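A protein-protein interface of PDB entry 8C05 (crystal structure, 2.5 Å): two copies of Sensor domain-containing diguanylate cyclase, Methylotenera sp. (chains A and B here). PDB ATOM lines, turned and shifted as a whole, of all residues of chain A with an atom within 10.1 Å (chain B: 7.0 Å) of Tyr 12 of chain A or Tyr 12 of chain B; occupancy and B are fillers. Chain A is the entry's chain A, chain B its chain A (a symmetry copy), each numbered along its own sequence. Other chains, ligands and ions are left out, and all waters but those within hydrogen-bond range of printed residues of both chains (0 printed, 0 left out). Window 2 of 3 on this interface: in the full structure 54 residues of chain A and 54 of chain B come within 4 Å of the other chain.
The side-chain carboxylate (OE1) of Glu 15 of chain A lies close to the side-chain carboxylate (OE1) of Glu 15 of chain B, at 3.4 Å.
O of Ile 109 of chain A lies within hydrogen-bond range of N of Thr 117 of chain A (3.1 Å). N of Ile 109 of chain A lies within hydrogen-bond range of O of His 118 of chain A (3.2 Å).
Tyr 12 of chain B touches Tyr 12 of chain A. Leu 13 of chain A touches Asn 111 of chain B (CB to OD1, 3.2 Å). CD2 of Leu 14 of chain A touches OE2 of Glu 15 of chain B, at 3.4 Å. Glu 15 of chain A touches Leu 14 of chain B. Ile 109 of chain B touches Ile 17 of chain A. Leu 14 of chain B touches Ile 27 of chain A. Ile 17 of chain B touches Ile 109 of chain A (CD1 to CG1, 3.7 Å). Leu 13 of chain B touches Ile 110 of chain A (CD2 to O, 3.1 Å). Asn 111 of chain A touches Leu 13 of chain B (OD1 to CB, 3.2 Å). CG2 of Ile 17 of chain B touches CD2 of Leu 120 of chain A, at 3.6 Å.
Tyr 12 of chain A touches just one residue of chain B: Tyr 12. Of chain A, only Tyr 12 (3.6 Å) comes within 4 Å of Tyr 12 of chain B. Of the printed residues of chain A, Leu 14 of chain B touches Glu 15, Ile 27 and Leu 120. Of the printed residues of chain B, Asn 111 of chain A touches Leu 13 (3.2 Å). Printed residues of chain A within 4 Å of Glu 15 of chain B: Leu 14 and Glu 15. Printed residues of chain A within 4 Å of Ile 17 of chain B: Ile 109 and Leu 120. Lys 112 of chain A touches none of the printed residues of chain B. The nearest residue of chain B that does not touch Tyr 12 of chain A is Asn 111 of chain B (4.1 Å). The nearest residue of chain A that does not touch Tyr 12 of chain B is Asn 111 of chain A (4.1 Å). The nearest printed residue of chain A that does not touch Asn 111 of chain B is Tyr 12 of chain A (4.1 Å).
Of the 9 printed residues of chain B, 7 touch a printed residue of chain A. Printed residues of chain A that touch a printed residue of chain B: Tyr 12, Leu 13, Leu 14, Glu 15, Ile 17, Ile 27, Ile 109, Ile 110, Asn 111 and Leu 120. Among the printed residues, no Asp or Glu carboxylate lies within 4 Å of a Lys or Arg side-chain nitrogen of the other chain.
Tyr 12 of chain A touches its own counterpart, Tyr 12 of chain B. Leu 14 of chain A touches Glu 15 of chain B, and with the chains exchanged Glu 15 of chain A touches Leu 14 of chain B. Glu 15 of chain A touches its own counterpart, Glu 15 of chain B. Ile 17 of chain A touches Ile 109 of chain B, and with the chains exchanged Ile 109 of chain A touches Ile 17 of chain B. Of the 12 pairs that touch across the chains among the printed residues, 8 have their exchanged pair printed and touching as well.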
ATOM      1  N   GLN A  11      23.759 -12.214  35.893  1.00  0.00           N
ATOM      2  CA  GLN A  11      23.237 -10.855  35.825  1.00  0.00           C
ATOM      3  C   GLN A  11      21.956 -10.802  34.996  1.00  0.00           C
ATOM      4  O   GLN A  11      21.989 -10.952  33.774  1.00  0.00           O
ATOM      5  CB  GLN A  11      24.284  -9.905  35.241  1.00  0.00           C
ATOM      6  N   TYR A  12      20.827 -10.588  35.671  1.00  0.00           N
ATOM      7  CA  TYR A  12      19.537 -10.521  34.996  1.00  0.00           C
ATOM      8  C   TYR A  12      19.181  -9.112  34.542  1.00  0.00           C
ATOM      9  O   TYR A  12      18.473  -8.954  33.539  1.00  0.00           O
ATOM     10  CB  TYR A  12      18.435 -11.066  35.909  1.00  0.00           C
ATOM     11  CG  TYR A  12      18.477 -12.569  36.087  1.00  0.00           C
ATOM     12  CD1 TYR A  12      19.230 -13.150  37.100  1.00  0.00           C
ATOM     13  CD2 TYR A  12      17.766 -13.408  35.238  1.00  0.00           C
ATOM     14  CE1 TYR A  12      19.271 -14.523  37.263  1.00  0.00           C
ATOM     15  CE2 TYR A  12      17.801 -14.781  35.393  1.00  0.00           C
ATOM     16  CZ  TYR A  12      18.554 -15.333  36.407  1.00  0.00           C
ATOM     17  OH  TYR A  12      18.591 -16.699  36.564  1.00  0.00           O
ATOM     18  N   LEU A  13      19.652  -8.084  35.255  1.00  0.00           N
ATOM     19  CA  LEU A  13      19.470  -6.712  34.797  1.00  0.00           C
ATOM     20  C   LEU A  13      20.175  -6.456  33.471  1.00  0.00           C
ATOM     21  O   LEU A  13      19.770  -5.551  32.735  1.00  0.00           O
ATOM     22  CB  LEU A  13      19.980  -5.726  35.851  1.00  0.00           C
ATOM     23  CG  LEU A  13      19.726  -4.241  35.571  1.00  0.00           C
ATOM     24  CD1 LEU A  13      18.244  -3.913  35.703  1.00  0.00           C
ATOM     25  CD2 LEU A  13      20.564  -3.352  36.474  1.00  0.00           C
ATOM     26  N   LEU A  14      21.215  -7.237  33.153  1.00  0.00           N
ATOM     27  CA  LEU A  14      21.917  -7.082  31.883  1.00  0.00           C
ATOM     28  C   LEU A  14      20.956  -7.100  30.703  1.00  0.00           C
ATOM     29  O   LEU A  14      21.185  -6.409  29.704  1.00  0.00           O
ATOM     30  CB  LEU A  14      22.971  -8.182  31.732  1.00  0.00           C
ATOM     31  CG  LEU A  14      23.799  -8.201  30.443  1.00  0.00           C
ATOM     32  CD1 LEU A  14      24.567  -6.900  30.271  1.00  0.00           C
ATOM     33  CD2 LEU A  14      24.748  -9.393  30.428  1.00  0.00           C
ATOM     34  N   GLU A  15      19.872  -7.872  30.803  1.00  0.00           N
ATOM     35  CA  GLU A  15      18.851  -7.861  29.761  1.00  0.00           C
ATOM     36  C   GLU A  15      18.238  -6.475  29.610  1.00  0.00           C
ATOM     37  O   GLU A  15      18.069  -5.975  28.491  1.00  0.00           O
ATOM     38  CB  GLU A  15      17.772  -8.896  30.079  1.00  0.00           C
ATOM     39  CG  GLU A  15      16.545  -8.811  29.186  1.00  0.00           C
ATOM     40  CD  GLU A  15      16.840  -9.191  27.750  1.00  0.00           C
ATOM     41  OE1 GLU A  15      17.701 -10.069  27.529  1.00  0.00           O
ATOM     42  OE2 GLU A  15      16.214  -8.608  26.841  1.00  0.00           O
ATOM     43  N   ALA A  16      17.905  -5.832  30.731  1.00  0.00           N
ATOM     44  CA  ALA A  16      17.280  -4.515  30.671  1.00  0.00           C
ATOM     45  C   ALA A  16      18.256  -3.445  30.199  1.00  0.00           C
ATOM     46  O   ALA A  16      17.847  -2.495  29.523  1.00  0.00           O
ATOM     47  CB  ALA A  16      16.705  -4.141  32.037  1.00  0.00           C
ATOM     48  N   ILE A  17      19.538  -3.575  30.542  1.00  0.00           N
ATOM     49  CA  ILE A  17      20.507  -2.556  30.149  1.00  0.00           C
ATOM     50  C   ILE A  17      20.833  -2.674  28.666  1.00  0.00           C
ATOM     51  O   ILE A  17      20.965  -1.665  27.963  1.00  0.00           O
ATOM     52  CB  ILE A  17      21.774  -2.653  31.017  1.00  0.00           C
ATOM     53  CG1 ILE A  17      21.403  -2.827  32.490  1.00  0.00           C
ATOM     54  CG2 ILE A  17      22.624  -1.406  30.846  1.00  0.00           C
ATOM     55  CD1 ILE A  17      22.602  -2.976  33.401  1.00  0.00           C
ATOM     56  N   VAL A  18      20.971  -3.905  28.166  1.00  0.00           N
ATOM     57  CA  VAL A  18      21.191  -4.103  26.737  1.00  0.00           C
ATOM     58  C   VAL A  18      19.949  -3.706  25.948  1.00  0.00           C
ATOM     59  O   VAL A  18      20.048  -3.282  24.789  1.00  0.00           O
ATOM     60  CB  VAL A  18      21.612  -5.559  26.461  1.00  0.00           C
ATOM     61  CG1 VAL A  18      21.727  -5.821  24.969  1.00  0.00           C
ATOM     62  CG2 VAL A  18      22.934  -5.862  27.143  1.00  0.00           C
ATOM     63  N   ARG A  19      18.766  -3.819  26.560  1.00  0.00           N
ATOM     64  CA  ARG A  19      17.543  -3.353  25.913  1.00  0.00           C
ATOM     65  C   ARG A  19      17.651  -1.891  25.502  1.00  0.00           C
ATOM     66  O   ARG A  19      17.111  -1.495  24.463  1.00  0.00           O
ATOM     67  CB  ARG A  19      16.349  -3.558  26.846  1.00  0.00           C
ATOM     68  CG  ARG A  19      15.012  -3.135  26.261  1.00  0.00           C
ATOM     69  CD  ARG A  19      13.903  -3.238  27.295  1.00  0.00           C
ATOM     70  NE  ARG A  19      14.042  -2.245  28.354  1.00  0.00           N
ATOM     71  CZ  ARG A  19      13.448  -1.059  28.350  1.00  0.00           C
ATOM     72  NH1 ARG A  19      12.664  -0.682  27.353  1.00  0.00           N
ATOM     73  NH2 ARG A  19      13.644  -0.232  29.373  1.00  0.00           N
ATOM     74  N   ILE A  27      10.552  -7.800  19.157  1.00  0.00           N
ATOM     75  CA  ILE A  27      10.099  -9.164  19.398  1.00  0.00           C
ATOM     76  C   ILE A  27       8.718  -9.310  18.779  1.00  0.00           C
ATOM     77  O   ILE A  27       7.839  -8.470  19.005  1.00  0.00           O
ATOM     78  CB  ILE A  27      10.062  -9.498  20.901  1.00  0.00           C
ATOM     79  CG1 ILE A  27      11.437  -9.285  21.533  1.00  0.00           C
ATOM     80  CG2 ILE A  27       9.603 -10.934  21.118  1.00  0.00           C
ATOM     81  CD1 ILE A  27      12.485 -10.238  21.022  1.00  0.00           C
ATOM     82  N   ILE A 109      13.411 -17.985  18.340  1.00  0.00           N
ATOM     83  CA  ILE A 109      13.574 -18.157  19.780  1.00  0.00           C
ATOM     84  C   ILE A 109      13.009 -19.522  20.150  1.00  0.00           C
ATOM     85  O   ILE A 109      11.810 -19.771  19.974  1.00  0.00           O
ATOM     86  CB  ILE A 109      12.879 -17.039  20.572  1.00  0.00           C
ATOM     87  CG1 ILE A 109      13.345 -15.668  20.081  1.00  0.00           C
ATOM     88  CG2 ILE A 109      13.151 -17.194  22.061  1.00  0.00           C
ATOM     89  CD1 ILE A 109      12.686 -14.506  20.790  1.00  0.00           C
ATOM     90  N   ILE A 110      13.869 -20.400  20.664  1.00  0.00           N
ATOM     91  CA  ILE A 110      13.512 -21.785  20.960  1.00  0.00           C
ATOM     92  C   ILE A 110      13.873 -22.067  22.413  1.00  0.00           C
ATOM     93  O   ILE A 110      15.056 -22.201  22.746  1.00  0.00           O
ATOM     94  CB  ILE A 110      14.218 -22.775  20.024  1.00  0.00           C
ATOM     95  CG1 ILE A 110      13.930 -22.429  18.560  1.00  0.00           C
ATOM     96  CG2 ILE A 110      13.790 -24.200  20.336  1.00  0.00           C
ATOM     97  CD1 ILE A 110      14.734 -23.243  17.569  1.00  0.00           C
ATOM     98  N   ASN A 111      12.860 -22.174  23.272  1.00  0.00           N
ATOM     99  CA  ASN A 111      13.049 -22.448  24.694  1.00  0.00           C
ATOM    100  C   ASN A 111      12.586 -23.870  24.991  1.00  0.00           C
ATOM    101  O   ASN A 111      11.388 -24.165  24.913  1.00  0.00           O
ATOM    102  CB  ASN A 111      12.291 -21.439  25.553  1.00  0.00           C
ATOM    103  CG  ASN A 111      13.147 -20.256  25.955  1.00  0.00           C
ATOM    104  OD1 ASN A 111      14.366 -20.373  26.074  1.00  0.00           O
ATOM    105  ND2 ASN A 111      12.511 -19.111  26.177  1.00  0.00           N
ATOM    106  N   LYS A 112      13.535 -24.741  25.341  1.00  0.00           N
ATOM    107  CA  LYS A 112      13.252 -26.132  25.698  1.00  0.00           C
ATOM    108  C   LYS A 112      12.437 -26.821  24.606  1.00  0.00           C
ATOM    109  O   LYS A 112      11.363 -27.377  24.849  1.00  0.00           O
ATOM    110  CB  LYS A 112      12.548 -26.215  27.053  1.00  0.00           C
ATOM    111  CG  LYS A 112      13.382 -25.676  28.204  1.00  0.00           C
ATOM    112  CD  LYS A 112      12.626 -25.718  29.520  1.00  0.00           C
ATOM    113  CE  LYS A 112      13.498 -25.222  30.660  1.00  0.00           C
ATOM    114  NZ  LYS A 112      14.006 -23.843  30.417  1.00  0.00           N
ATOM    115  N   THR A 117       8.806 -19.821  19.211  1.00  0.00           N
ATOM    116  CA  THR A 117       7.766 -19.145  19.979  1.00  0.00           C
ATOM    117  C   THR A 117       7.666 -17.677  19.585  1.00  0.00           C
ATOM    118  O   THR A 117       6.563 -17.128  19.476  1.00  0.00           O
ATOM    119  CB  THR A 117       8.036 -19.280  21.479  1.00  0.00           C
ATOM    120  OG1 THR A 117       9.360 -18.818  21.773  1.00  0.00           O
ATOM    121  CG2 THR A 117       7.895 -20.732  21.922  1.00  0.00           C
ATOM    122  N   HIS A 118       8.808 -17.028  19.354  1.00  0.00           N
ATOM    123  CA  HIS A 118       8.847 -15.645  18.900  1.00  0.00           C
ATOM    124  C   HIS A 118       9.995 -15.483  17.913  1.00  0.00           C
ATOM    125  O   HIS A 118      10.733 -16.430  17.621  1.00  0.00           O
ATOM    126  CB  HIS A 118       8.992 -14.676  20.079  1.00  0.00           C
ATOM    127  CG  HIS A 118       7.860 -14.739  21.057  1.00  0.00           C
ATOM    128  ND1 HIS A 118       7.783 -15.695  22.045  1.00  0.00           N
ATOM    129  CD2 HIS A 118       6.758 -13.964  21.196  1.00  0.00           C
ATOM    130  CE1 HIS A 118       6.683 -15.507  22.753  1.00  0.00           C
ATOM    131  NE2 HIS A 118       6.044 -14.461  22.258  1.00  0.00           N
ATOM    132  N   LEU A 120      13.229 -12.617  16.818  1.00  0.00           N
ATOM    133  CA  LEU A 120      14.037 -11.483  17.251  1.00  0.00           C
ATOM    134  C   LEU A 120      14.480 -10.682  16.034  1.00  0.00           C
ATOM    135  O   LEU A 120      15.138 -11.222  15.139  1.00  0.00           O
ATOM    136  CB  LEU A 120      15.254 -11.947  18.051  1.00  0.00           C
ATOM    137  CG  LEU A 120      16.255 -10.842  18.399  1.00  0.00           C
ATOM    138  CD1 LEU A 120      15.593  -9.782  19.261  1.00  0.00           C
ATOM    139  CD2 LEU A 120      17.491 -11.403  19.088  1.00  0.00           C
ATOM    140  N   GLN B  11      11.040 -14.380  28.263  1.00  0.00           N
ATOM    141  CA  GLN B  11      12.005 -15.045  27.396  1.00  0.00           C
ATOM    142  C   GLN B  11      13.425 -14.878  27.929  1.00  0.00           C
ATOM    143  O   GLN B  11      13.993 -13.786  27.883  1.00  0.00           O
ATOM    144  CB  GLN B  11      11.910 -14.501  25.969  1.00  0.00           C
ATOM    145  N   TYR B  12      13.994 -15.971  28.439  1.00  0.00           N
ATOM    146  CA  TYR B  12      15.345 -15.943  28.985  1.00  0.00           C
ATOM    147  C   TYR B  12      16.411 -16.238  27.939  1.00  0.00           C
ATOM    148  O   TYR B  12      17.537 -15.740  28.058  1.00  0.00           O
ATOM    149  CB  TYR B  12      15.465 -16.936  30.144  1.00  0.00           C
ATOM    150  CG  TYR B  12      14.744 -16.499  31.402  1.00  0.00           C
ATOM    151  CD1 TYR B  12      13.411 -16.828  31.613  1.00  0.00           C
ATOM    152  CD2 TYR B  12      15.397 -15.753  32.375  1.00  0.00           C
ATOM    153  CE1 TYR B  12      12.750 -16.428  32.761  1.00  0.00           C
ATOM    154  CE2 TYR B  12      14.744 -15.349  33.524  1.00  0.00           C
ATOM    155  CZ  TYR B  12      13.421 -15.689  33.713  1.00  0.00           C
ATOM    156  OH  TYR B  12      12.769 -15.288  34.855  1.00  0.00           O
ATOM    157  N   LEU B  13      16.085 -17.038  26.918  1.00  0.00           N
ATOM    158  CA  LEU B  13      17.009 -17.246  25.810  1.00  0.00           C
ATOM    159  C   LEU B  13      17.291 -15.955  25.052  1.00  0.00           C
ATOM    160  O   LEU B  13      18.345 -15.843  24.418  1.00  0.00           O
ATOM    161  CB  LEU B  13      16.456 -18.300  24.846  1.00  0.00           C
ATOM    162  CG  LEU B  13      17.384 -18.729  23.704  1.00  0.00           C
ATOM    163  CD1 LEU B  13      18.550 -19.551  24.237  1.00  0.00           C
ATOM    164  CD2 LEU B  13      16.627 -19.489  22.628  1.00  0.00           C
ATOM    165  N   LEU B  14      16.374 -14.982  25.110  1.00  0.00           N
ATOM    166  CA  LEU B  14      16.588 -13.700  24.445  1.00  0.00           C
ATOM    167  C   LEU B  14      17.928 -13.086  24.824  1.00  0.00           C
ATOM    168  O   LEU B  14      18.563 -12.423  23.998  1.00  0.00           O
ATOM    169  CB  LEU B  14      15.445 -12.739  24.785  1.00  0.00           C
ATOM    170  CG  LEU B  14      15.506 -11.326  24.196  1.00  0.00           C
ATOM    171  CD1 LEU B  14      15.539 -11.371  22.676  1.00  0.00           C
ATOM    172  CD2 LEU B  14      14.333 -10.486  24.685  1.00  0.00           C
ATOM    173  N   GLU B  15      18.380 -13.307  26.060  1.00  0.00           N
ATOM    174  CA  GLU B  15      19.703 -12.844  26.464  1.00  0.00           C
ATOM    175  C   GLU B  15      20.791 -13.486  25.613  1.00  0.00           C
ATOM    176  O   GLU B  15      21.712 -12.806  25.143  1.00  0.00           O
ATOM    177  CB  GLU B  15      19.930 -13.146  27.945  1.00  0.00           C
ATOM    178  CG  GLU B  15      21.357 -12.916  28.416  1.00  0.00           C
ATOM    179  CD  GLU B  15      21.752 -11.454  28.394  1.00  0.00           C
ATOM    180  OE1 GLU B  15      20.878 -10.596  28.642  1.00  0.00           O
ATOM    181  OE2 GLU B  15      22.936 -11.163  28.126  1.00  0.00           O
ATOM    182  N   ALA B  16      20.696 -14.799  25.395  1.00  0.00           N
ATOM    183  CA  ALA B  16      21.717 -15.495  24.619  1.00  0.00           C
ATOM    184  C   ALA B  16      21.663 -15.120  23.144  1.00  0.00           C
ATOM    185  O   ALA B  16      22.705 -15.076  22.481  1.00  0.00           O
ATOM    186  CB  ALA B  16      21.566 -17.007  24.786  1.00  0.00           C
ATOM    187  N   ILE B  17      20.469 -14.850  22.612  1.00  0.00           N
ATOM    188  CA  ILE B  17      20.358 -14.523  21.193  1.00  0.00           C
ATOM    189  C   ILE B  17      20.860 -13.109  20.931  1.00  0.00           C
ATOM    190  O   ILE B  17      21.535 -12.851  19.927  1.00  0.00           O
ATOM    191  CB  ILE B  17      18.911 -14.711  20.708  1.00  0.00           C
ATOM    192  CG1 ILE B  17      18.333 -16.023  21.238  1.00  0.00           C
ATOM    193  CG2 ILE B  17      18.860 -14.704  19.191  1.00  0.00           C
ATOM    194  CD1 ILE B  17      16.892 -16.254  20.838  1.00  0.00           C
ATOM    195  N   ILE B 109      25.851  -1.609  36.389  1.00  0.00           N
ATOM    196  CA  ILE B 109      24.893  -2.684  36.628  1.00  0.00           C
ATOM    197  C   ILE B 109      24.577  -2.700  38.118  1.00  0.00           C
ATOM    198  O   ILE B 109      25.469  -2.934  38.943  1.00  0.00           O
ATOM    199  CB  ILE B 109      25.433  -4.046  36.164  1.00  0.00           C
ATOM    200  CG1 ILE B 109      25.889  -3.969  34.706  1.00  0.00           C
ATOM    201  CG2 ILE B 109      24.374  -5.124  36.336  1.00  0.00           C
ATOM    202  CD1 ILE B 109      26.464  -5.264  34.176  1.00  0.00           C
ATOM    203  N   ASN B 111      21.973  -4.365  40.810  1.00  0.00           N
ATOM    204  CA  ASN B 111      20.965  -5.376  41.119  1.00  0.00           C
ATOM    205  C   ASN B 111      20.590  -5.269  42.592  1.00  0.00           C
ATOM    206  O   ASN B 111      21.410  -5.567  43.468  1.00  0.00           O
ATOM    207  CB  ASN B 111      21.474  -6.777  40.787  1.00  0.00           C
ATOM    208  CG  ASN B 111      21.088  -7.223  39.392  1.00  0.00           C
ATOM    209  OD1 ASN B 111      20.067  -6.795  38.855  1.00  0.00           O
ATOM    210  ND2 ASN B 111      21.898  -8.094  38.802  1.00  0.00           N
